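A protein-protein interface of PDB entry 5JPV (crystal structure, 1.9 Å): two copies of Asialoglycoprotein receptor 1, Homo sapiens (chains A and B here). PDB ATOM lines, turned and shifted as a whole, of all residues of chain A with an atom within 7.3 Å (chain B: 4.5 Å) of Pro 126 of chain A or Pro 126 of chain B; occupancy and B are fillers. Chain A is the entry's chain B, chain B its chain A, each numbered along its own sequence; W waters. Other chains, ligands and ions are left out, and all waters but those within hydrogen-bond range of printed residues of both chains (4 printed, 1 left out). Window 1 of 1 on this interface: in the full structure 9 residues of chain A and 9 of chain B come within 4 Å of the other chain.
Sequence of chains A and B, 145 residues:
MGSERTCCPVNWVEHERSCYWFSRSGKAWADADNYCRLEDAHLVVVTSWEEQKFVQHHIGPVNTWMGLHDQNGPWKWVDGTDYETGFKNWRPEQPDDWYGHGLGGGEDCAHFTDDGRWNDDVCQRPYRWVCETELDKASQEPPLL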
ATOM      1  N   SER A  25     -15.783 -11.254  19.891  1.00  0.00           N
ATOM      2  CA  SER A  25     -16.623 -10.677  18.854  1.00  0.00           C
ATOM      3  C   SER A  25     -16.162 -11.274  17.534  1.00  0.00           C
ATOM      4  O   SER A  25     -15.097 -11.909  17.470  1.00  0.00           O
ATOM      5  CB  SER A  25     -16.437  -9.162  18.814  1.00  0.00           C
ATOM      6  OG  SER A  25     -15.073  -8.864  18.579  1.00  0.00           O
ATOM      7  N   GLY A  26     -16.941 -11.064  16.481  1.00  0.00           N
ATOM      8  CA  GLY A  26     -16.631 -11.667  15.186  1.00  0.00           C
ATOM      9  C   GLY A  26     -16.208 -10.692  14.112  1.00  0.00           C
ATOM     10  O   GLY A  26     -16.603  -9.530  14.128  1.00  0.00           O
ATOM     11  N   LYS A  27     -15.399 -11.176  13.174  1.00  0.00           N
ATOM     12  CA  LYS A  27     -14.951 -10.389  12.028  1.00  0.00           C
ATOM     13  C   LYS A  27     -14.828 -11.308  10.814  1.00  0.00           C
ATOM     14  O   LYS A  27     -14.530 -12.503  10.966  1.00  0.00           O
ATOM     15  CB  LYS A  27     -13.578  -9.753  12.302  1.00  0.00           C
ATOM     16  CG  LYS A  27     -13.582  -8.463  13.130  1.00  0.00           C
ATOM     17  CD  LYS A  27     -12.154  -7.929  13.303  1.00  0.00           C
ATOM     18  CE  LYS A  27     -12.093  -6.690  14.207  1.00  0.00           C
ATOM     19  NZ  LYS A  27     -12.590  -5.466  13.520  1.00  0.00           N
ATOM     20  N   ALA A  28     -15.031 -10.759   9.614  1.00  0.00           N
ATOM     21  CA  ALA A  28     -14.613 -11.459   8.389  1.00  0.00           C
ATOM     22  C   ALA A  28     -13.109 -11.783   8.480  1.00  0.00           C
ATOM     23  O   ALA A  28     -12.369 -11.106   9.195  1.00  0.00           O
ATOM     24  CB  ALA A  28     -14.917 -10.619   7.147  1.00  0.00           C
ATOM     25  N   TRP A  29     -12.655 -12.822   7.782  1.00  0.00           N
ATOM     26  CA  TRP A  29     -11.254 -13.241   7.909  1.00  0.00           C
ATOM     27  C   TRP A  29     -10.271 -12.090   7.626  1.00  0.00           C
ATOM     28  O   TRP A  29      -9.365 -11.838   8.414  1.00  0.00           O
ATOM     29  CB  TRP A  29     -10.959 -14.438   6.992  1.00  0.00           C
ATOM     30  CG  TRP A  29      -9.622 -15.105   7.240  1.00  0.00           C
ATOM     31  CD1 TRP A  29      -9.394 -16.214   7.988  1.00  0.00           C
ATOM     32  CD2 TRP A  29      -8.348 -14.724   6.685  1.00  0.00           C
ATOM     33  NE1 TRP A  29      -8.052 -16.544   7.957  1.00  0.00           N
ATOM     34  CE2 TRP A  29      -7.390 -15.641   7.169  1.00  0.00           C
ATOM     35  CE3 TRP A  29      -7.927 -13.684   5.841  1.00  0.00           C
ATOM     36  CZ2 TRP A  29      -6.030 -15.556   6.836  1.00  0.00           C
ATOM     37  CZ3 TRP A  29      -6.573 -13.588   5.519  1.00  0.00           C
ATOM     38  CH2 TRP A  29      -5.640 -14.525   6.017  1.00  0.00           C
ATOM     39  N   ASN A  63     -16.953 -21.522  16.349  1.00  0.00           N
ATOM     40  CA  ASN A  63     -16.237 -21.315  15.086  1.00  0.00           C
ATOM     41  C   ASN A  63     -15.324 -20.103  15.207  1.00  0.00           C
ATOM     42  O   ASN A  63     -15.774 -19.014  15.571  1.00  0.00           O
ATOM     43  CB  ASN A  63     -17.208 -21.148  13.910  1.00  0.00           C
ATOM     44  CG  ASN A  63     -17.926 -22.440  13.547  1.00  0.00           C
ATOM     45  OD1 ASN A  63     -19.126 -22.434  13.262  1.00  0.00           O
ATOM     46  ND2 ASN A  63     -17.199 -23.553  13.560  1.00  0.00           N
ATOM     47  N   TRP A  65     -11.697 -18.211  13.484  1.00  0.00           N
ATOM     48  CA  TRP A  65     -10.712 -18.081  12.404  1.00  0.00           C
ATOM     49  C   TRP A  65      -9.286 -18.364  12.887  1.00  0.00           C
ATOM     50  O   TRP A  65      -8.920 -17.986  14.002  1.00  0.00           O
ATOM     51  CB  TRP A  65     -10.733 -16.654  11.845  1.00  0.00           C
ATOM     52  CG  TRP A  65     -11.917 -16.277  10.981  1.00  0.00           C
ATOM     53  CD1 TRP A  65     -12.674 -15.141  11.087  1.00  0.00           C
ATOM     54  CD2 TRP A  65     -12.446 -17.006   9.865  1.00  0.00           C
ATOM     55  NE1 TRP A  65     -13.648 -15.125  10.119  1.00  0.00           N
ATOM     56  CE2 TRP A  65     -13.530 -16.256   9.354  1.00  0.00           C
ATOM     57  CE3 TRP A  65     -12.121 -18.231   9.257  1.00  0.00           C
ATOM     58  CZ2 TRP A  65     -14.280 -16.678   8.255  1.00  0.00           C
ATOM     59  CZ3 TRP A  65     -12.880 -18.656   8.167  1.00  0.00           C
ATOM     60  CH2 TRP A  65     -13.947 -17.879   7.679  1.00  0.00           C
ATOM     61  N   HIS A 101     -22.779 -22.963  -0.998  1.00  0.00           N
ATOM     62  CA  HIS A 101     -23.325 -21.911  -0.143  1.00  0.00           C
ATOM     63  C   HIS A 101     -23.931 -20.790  -0.986  1.00  0.00           C
ATOM     64  O   HIS A 101     -24.725 -19.994  -0.490  1.00  0.00           O
ATOM     65  CB  HIS A 101     -22.230 -21.344   0.771  1.00  0.00           C
ATOM     66  CG  HIS A 101     -20.980 -20.984   0.043  1.00  0.00           C
ATOM     67  ND1 HIS A 101     -20.851 -19.827  -0.694  1.00  0.00           N
ATOM     68  CD2 HIS A 101     -19.806 -21.644  -0.084  1.00  0.00           C
ATOM     69  CE1 HIS A 101     -19.652 -19.790  -1.243  1.00  0.00           C
ATOM     70  NE2 HIS A 101     -18.996 -20.880  -0.884  1.00  0.00           N
ATOM     71  N   LEU A 103     -22.673 -18.076  -2.174  1.00  0.00           N
ATOM     72  CA  LEU A 103     -22.251 -16.708  -1.854  1.00  0.00           C
ATOM     73  C   LEU A 103     -21.195 -16.163  -2.816  1.00  0.00           C
ATOM     74  O   LEU A 103     -20.812 -14.994  -2.734  1.00  0.00           O
ATOM     75  CB  LEU A 103     -21.727 -16.631  -0.416  1.00  0.00           C
ATOM     76  CG  LEU A 103     -22.646 -16.344   0.782  1.00  0.00           C
ATOM     77  CD1 LEU A 103     -24.162 -16.378   0.492  1.00  0.00           C
ATOM     78  CD2 LEU A 103     -22.260 -17.245   1.933  1.00  0.00           C
ATOM     79  N   VAL A 122     -16.175 -19.721   3.903  1.00  0.00           N
ATOM     80  CA  VAL A 122     -16.204 -18.484   3.134  1.00  0.00           C
ATOM     81  C   VAL A 122     -15.566 -17.373   3.963  1.00  0.00           C
ATOM     82  O   VAL A 122     -15.979 -17.126   5.099  1.00  0.00           O
ATOM     83  CB  VAL A 122     -17.649 -18.131   2.746  1.00  0.00           C
ATOM     84  CG1 VAL A 122     -17.696 -16.870   1.919  1.00  0.00           C
ATOM     85  CG2 VAL A 122     -18.275 -19.292   1.960  1.00  0.00           C
ATOM     86  N   CYS A 123     -14.560 -16.714   3.388  1.00  0.00           N
ATOM     87  CA  CYS A 123     -13.736 -15.747   4.125  1.00  0.00           C
ATOM     88  C   CYS A 123     -14.519 -14.563   4.711  1.00  0.00           C
ATOM     89  O   CYS A 123     -14.141 -14.022   5.757  1.00  0.00           O
ATOM     90  CB  CYS A 123     -12.583 -15.260   3.254  1.00  0.00           C
ATOM     91  SG  CYS A 123     -11.442 -16.593   2.795  1.00  0.00           S
ATOM     92  N   GLN A 124     -15.608 -14.173   4.056  1.00  0.00           N
ATOM     93  CA  GLN A 124     -16.427 -13.052   4.558  1.00  0.00           C
ATOM     94  C   GLN A 124     -17.332 -13.340   5.768  1.00  0.00           C
ATOM     95  O   GLN A 124     -17.909 -12.408   6.324  1.00  0.00           O
ATOM     96  CB  GLN A 124     -17.194 -12.313   3.437  1.00  0.00           C
ATOM     97  CG  GLN A 124     -17.861 -13.166   2.383  1.00  0.00           C
ATOM     98  CD  GLN A 124     -18.569 -12.348   1.298  1.00  0.00           C
ATOM     99  OE1 GLN A 124     -18.856 -11.165   1.472  1.00  0.00           O
ATOM    100  NE2 GLN A 124     -18.860 -12.990   0.182  1.00  0.00           N
ATOM    101  N   ARG A 125     -17.439 -14.603   6.189  1.00  0.00           N
ATOM    102  CA  ARG A 125     -18.239 -14.949   7.376  1.00  0.00           C
ATOM    103  C   ARG A 125     -17.628 -14.336   8.628  1.00  0.00           C
ATOM    104  O   ARG A 125     -16.420 -14.444   8.829  1.00  0.00           O
ATOM    105  CB  ARG A 125     -18.347 -16.461   7.584  1.00  0.00           C
ATOM    106  CG  ARG A 125     -19.107 -17.205   6.492  1.00  0.00           C
ATOM    107  CD  ARG A 125     -19.693 -18.512   7.000  1.00  0.00           C
ATOM    108  NE  ARG A 125     -20.138 -19.349   5.885  1.00  0.00           N
ATOM    109  CZ  ARG A 125     -21.315 -19.221   5.281  1.00  0.00           C
ATOM    110  NH1 ARG A 125     -22.185 -18.301   5.703  1.00  0.00           N
ATOM    111  NH2 ARG A 125     -21.627 -20.017   4.266  1.00  0.00           N
ATOM    112  N   PRO A 126     -18.461 -13.705   9.478  1.00  0.00           N
ATOM    113  CA  PRO A 126     -17.955 -13.199  10.751  1.00  0.00           C
ATOM    114  C   PRO A 126     -17.833 -14.307  11.788  1.00  0.00           C
ATOM    115  O   PRO A 126     -18.843 -14.879  12.235  1.00  0.00           O
ATOM    116  CB  PRO A 126     -19.015 -12.167  11.172  1.00  0.00           C
ATOM    117  CG  PRO A 126     -20.279 -12.649  10.549  1.00  0.00           C
ATOM    118  CD  PRO A 126     -19.878 -13.343   9.261  1.00  0.00           C
ATOM    119  N   TYR A 127     -16.592 -14.607  12.164  1.00  0.00           N
ATOM    120  CA  TYR A 127     -16.317 -15.558  13.222  1.00  0.00           C
ATOM    121  C   TYR A 127     -15.388 -14.868  14.215  1.00  0.00           C
ATOM    122  O   TYR A 127     -14.686 -13.899  13.871  1.00  0.00           O
ATOM    123  CB  TYR A 127     -15.595 -16.805  12.664  1.00  0.00           C
ATOM    124  CG  TYR A 127     -16.429 -17.804  11.860  1.00  0.00           C
ATOM    125  CD1 TYR A 127     -17.770 -18.062  12.172  1.00  0.00           C
ATOM    126  CD2 TYR A 127     -15.842 -18.541  10.823  1.00  0.00           C
ATOM    127  CE1 TYR A 127     -18.519 -19.010  11.437  1.00  0.00           C
ATOM    128  CE2 TYR A 127     -16.584 -19.484  10.078  1.00  0.00           C
ATOM    129  CZ  TYR A 127     -17.918 -19.715  10.402  1.00  0.00           C
ATOM    130  OH  TYR A 127     -18.644 -20.647   9.678  1.00  0.00           O
ATOM    131  N   ARG A 128     -15.361 -15.375  15.442  1.00  0.00           N
ATOM    132  CA  ARG A 128     -14.324 -14.974  16.384  1.00  0.00           C
ATOM    133  C   ARG A 128     -12.961 -15.338  15.797  1.00  0.00           C
ATOM    134  O   ARG A 128     -12.880 -16.070  14.808  1.00  0.00           O
ATOM    135  CB  ARG A 128     -14.539 -15.629  17.742  1.00  0.00           C
ATOM    136  CG  ARG A 128     -15.809 -15.126  18.446  1.00  0.00           C
ATOM    137  CD  ARG A 128     -15.940 -15.647  19.845  1.00  0.00           C
ATOM    138  NE  ARG A 128     -17.124 -15.077  20.478  1.00  0.00           N
ATOM    139  CZ  ARG A 128     -17.464 -15.245  21.748  1.00  0.00           C
ATOM    140  NH1 ARG A 128     -16.708 -15.974  22.561  1.00  0.00           N
ATOM    141  NH2 ARG A 128     -18.570 -14.678  22.209  1.00  0.00           N
ATOM    142  N   GLY B  26     -23.059 -13.378  -2.262  1.00  0.00           N
ATOM    143  CA  GLY B  26     -23.340 -12.723  -0.983  1.00  0.00           C
ATOM    144  C   GLY B  26     -22.467 -11.537  -0.631  1.00  0.00           C
ATOM    145  O   GLY B  26     -21.313 -11.452  -1.058  1.00  0.00           O
ATOM    146  N   LYS B  27     -23.030 -10.632   0.166  1.00  0.00           N
ATOM    147  CA  LYS B  27     -22.327  -9.480   0.728  1.00  0.00           C
ATOM    148  C   LYS B  27     -22.863  -9.208   2.137  1.00  0.00           C
ATOM    149  O   LYS B  27     -24.021  -9.518   2.429  1.00  0.00           O
ATOM    150  CB  LYS B  27     -22.571  -8.231  -0.128  1.00  0.00           C
ATOM    151  CG  LYS B  27     -21.611  -8.027  -1.320  1.00  0.00           C
ATOM    152  CD  LYS B  27     -21.978  -6.759  -2.100  1.00  0.00           C
ATOM    153  CE  LYS B  27     -21.152  -6.611  -3.385  1.00  0.00           C
ATOM    154  NZ  LYS B  27     -19.722  -6.344  -3.095  1.00  0.00           N
ATOM    155  N   ALA B  28     -22.033  -8.613   2.997  1.00  0.00           N
ATOM    156  CA  ALA B  28     -22.520  -7.996   4.242  1.00  0.00           C
ATOM    157  C   ALA B  28     -23.524  -6.881   3.921  1.00  0.00           C
ATOM    158  O   ALA B  28     -23.469  -6.282   2.837  1.00  0.00           O
ATOM    159  CB  ALA B  28     -21.350  -7.445   5.069  1.00  0.00           C
ATOM    160  N   LEU B 103     -21.105 -12.593  18.303  1.00  0.00           N
ATOM    161  CA  LEU B 103     -20.269 -11.875  17.331  1.00  0.00           C
ATOM    162  C   LEU B 103     -20.146 -10.383  17.658  1.00  0.00           C
ATOM    163  O   LEU B 103     -19.406  -9.657  16.999  1.00  0.00           O
ATOM    164  CB  LEU B 103     -20.830 -12.058  15.912  1.00  0.00           C
ATOM    165  CG  LEU B 103     -20.465 -13.266  15.022  1.00  0.00           C
ATOM    166  CD1 LEU B 103     -19.711 -14.400  15.704  1.00  0.00           C
ATOM    167  CD2 LEU B 103     -21.698 -13.777  14.277  1.00  0.00           C
ATOM    168  N   GLN B 124     -23.063  -8.025   9.511  1.00  0.00           N
ATOM    169  CA  GLN B 124     -21.839  -8.579   8.895  1.00  0.00           C
ATOM    170  C   GLN B 124     -22.015  -9.860   8.078  1.00  0.00           C
ATOM    171  O   GLN B 124     -21.132 -10.216   7.290  1.00  0.00           O
ATOM    172  CB  GLN B 124     -20.794  -8.903   9.957  1.00  0.00           C
ATOM    173  CG  GLN B 124     -20.523  -7.843  10.990  1.00  0.00           C
ATOM    174  CD  GLN B 124     -19.420  -8.286  11.917  1.00  0.00           C
ATOM    175  OE1 GLN B 124     -18.264  -8.345  11.515  1.00  0.00           O
ATOM    176  NE2 GLN B 124     -19.770  -8.624  13.155  1.00  0.00           N
ATOM    177  N   ARG B 125     -23.103 -10.588   8.293  1.00  0.00           N
ATOM    178  CA  ARG B 125     -23.284 -11.855   7.585  1.00  0.00           C
ATOM    179  C   ARG B 125     -23.377 -11.661   6.076  1.00  0.00           C
ATOM    180  O   ARG B 125     -24.067 -10.754   5.614  1.00  0.00           O
ATOM    181  CB  ARG B 125     -24.518 -12.599   8.092  1.00  0.00           C
ATOM    182  CG  ARG B 125     -24.424 -13.016   9.555  1.00  0.00           C
ATOM    183  CD  ARG B 125     -25.404 -14.153   9.861  1.00  0.00           C
ATOM    184  NE  ARG B 125     -25.540 -14.390  11.297  1.00  0.00           N
ATOM    185  CZ  ARG B 125     -24.664 -15.069  12.037  1.00  0.00           C
ATOM    186  NH1 ARG B 125     -23.560 -15.583  11.485  1.00  0.00           N
ATOM    187  NH2 ARG B 125     -24.888 -15.232  13.331  1.00  0.00           N
ATOM    188  N   PRO B 126     -22.666 -12.503   5.304  1.00  0.00           N
ATOM    189  CA  PRO B 126     -22.832 -12.458   3.854  1.00  0.00           C
ATOM    190  C   PRO B 126     -24.086 -13.201   3.399  1.00  0.00           C
ATOM    191  O   PRO B 126     -24.173 -14.422   3.554  1.00  0.00           O
ATOM    192  CB  PRO B 126     -21.574 -13.156   3.325  1.00  0.00           C
ATOM    193  CG  PRO B 126     -21.134 -14.053   4.414  1.00  0.00           C
ATOM    194  CD  PRO B 126     -21.645 -13.482   5.724  1.00  0.00           C
ATOM    195  N   TYR B 127     -25.041 -12.460   2.848  1.00  0.00           N
ATOM    196  CA  TYR B 127     -26.243 -13.042   2.258  1.00  0.00           C
ATOM    197  C   TYR B 127     -26.406 -12.480   0.853  1.00  0.00           C
ATOM    198  O   TYR B 127     -25.860 -11.414   0.533  1.00  0.00           O
ATOM    199  CB  TYR B 127     -27.487 -12.663   3.080  1.00  0.00           C
ATOM    200  CG  TYR B 127     -27.675 -13.359   4.418  1.00  0.00           C
ATOM    201  CD1 TYR B 127     -27.272 -14.686   4.619  1.00  0.00           C
ATOM    202  CD2 TYR B 127     -28.317 -12.698   5.468  1.00  0.00           C
ATOM    203  CE1 TYR B 127     -27.474 -15.324   5.846  1.00  0.00           C
ATOM    204  CE2 TYR B 127     -28.518 -13.323   6.704  1.00  0.00           C
ATOM    205  CZ  TYR B 127     -28.098 -14.637   6.878  1.00  0.00           C
ATOM    206  OH  TYR B 127     -28.316 -15.242   8.086  1.00  0.00           O
HETATM  207  O   HOH W   1     -15.687  -8.071   9.610  1.00  0.00           O
HETATM  208  O   HOH W   2     -18.722  -9.967   6.363  1.00  0.00           O
HETATM  209  O   HOH W   3     -21.125 -16.689  12.454  1.00  0.00           O
HETATM  210  O   HOH W   4     -24.448 -16.811   4.648  1.00  0.00           O
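N of Gly 26 of chain B lies within hydrogen-bond range of O of Leu 103 of chain A (2.8 Å). The side-chain amide nitrogen (NE2) of Gln 124 of chain A lies within hydrogen-bond range of the backbone carbonyl oxygen (O) of Gly 26 of chain B, at 3.1 Å. N of Gly 26 of chain A sits at hydrogen-bond distance from O of Leu 103 of chain B, 2.9 Å away. OE1 of Gln 124 of chain B sits close to O of Gly 26 of chain A, at 3.3 Å.
Leu 103 of chain B touches Ser 25 of chain A. Gln 124 of chain B touches Lys 27 of chain A (OE1 to CA, 3.9 Å). Leu 103 of chain A touches Pro 126 of chain B (CD1 to O, 3.6 Å). Gln 124 of chain A touches Lys 27 of chain B. Gln 124 of chain A touches Pro 126 of chain B (CD to CB, 3.7 Å). Pro 126 of chain A touches Leu 103 of chain B (O to CG, 3.6 Å). CG of Pro 126 of chain A touches CB of Gln 124 of chain B, at 3.8 Å. CD of Pro 126 of chain A touches CD of Pro 126 of chain B (3.96 Å).
Water W2 bridges O of Gln 124 of chain A (2.6 Å) and O of Gln 124 of chain B (2.6 Å). Water W4 lies within hydrogen-bond range of the backbone carbonyl oxygen of Pro 126 of chain B and the guanidinium group of Arg 125 of chain A. Water W1 bridges N of Ala 28 of chain A and OE1 of Gln 124 of chain B. Water W3 bridges the guanidinium group (NH1) of Arg 125 of chain B (2.8 Å) and the backbone carbonyl oxygen (O) of Pro 126 of chain A (2.9 Å).
Gly 26 of chain A touches Leu 103 of chain B, and with the chains exchanged Leu 103 of chain A touches Gly 26 of chain B. Gly 26 of chain A touches Gln 124 of chain B, and with the chains exchanged Gln 124 of chain A touches Gly 26 of chain B. Leu 103 of chain A touches Pro 126 of chain B, and with the chains exchanged Pro 126 of chain A touches Leu 103 of chain B. Gln 124 of chain A touches Pro 126 of chain B, and with the chains exchanged Pro 126 of chain A touches Gln 124 of chain B. Positions printed for both chains: 26, 27, 28, 103, 124, 125, 126 and 127. Of the 12 pairs that touch across the chains among the printed residues, 11 have their exchanged pair printed and touching as well.
N of Lys 27 of chain B lies within hydrogen-bond range of O of Tyr 127 of chain B. The backbone carbonyl oxygen (O) of Lys 27 of chain A sits at hydrogen-bond distance from the indole nitrogen (NE1) of Trp 65 of chain A. The backbone carbonyl oxygen (O) of Tyr 127 of chain A sits at hydrogen-bond distance from the backbone NH (N) of Lys 27 of chain A (2.9 Å). The backbone NH of Leu 103 of chain A lies within hydrogen-bond range of a ring nitrogen (ND1) of His 101 of chain A (2.9 Å).
Of the 16 printed residues of chain A, 6 touch a printed residue of chain B. Hydrophobic or aromatic side chains of chain A that line the printed part of chain B: Leu 103 and Pro 126. Of the 8 printed residues of chain B, 5 touch a printed residue of chain A. Hydrophobic or aromatic side chains of chain B that line the printed part of chain A: Leu 103 and Pro 126. Among the printed residues, 12 pairs touch across the chains.
Pro 126 of chain A touches just these residues of chain B: Leu 103 (3.6 Å), Gln 124 (3.8 Å) and Pro 126 (3.96 Å). Pro 126 of chain B touches just these residues of chain A: Leu 103, Gln 124 and Pro 126. Of the printed residues of chain A, Leu 103 of chain B touches Ser 25, Gly 26 and Pro 126. Of the printed residues of chain B, Leu 103 of chain A touches Gly 26 and Pro 126. Printed residues of chain B within 4 Å of Lys 27 of chain A: Gln 124. Asn 63 of chain A touches none of the printed residues of chain B. Tyr 127 of chain A touches none of the printed residues of chain B. The nearest residue of chain B that does not touch Pro 126 of chain A is Arg 125 of chain B (4.1 Å). The nearest residue of chain A that does not touch Pro 126 of chain B is Arg 125 of chain A (4.1 Å).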
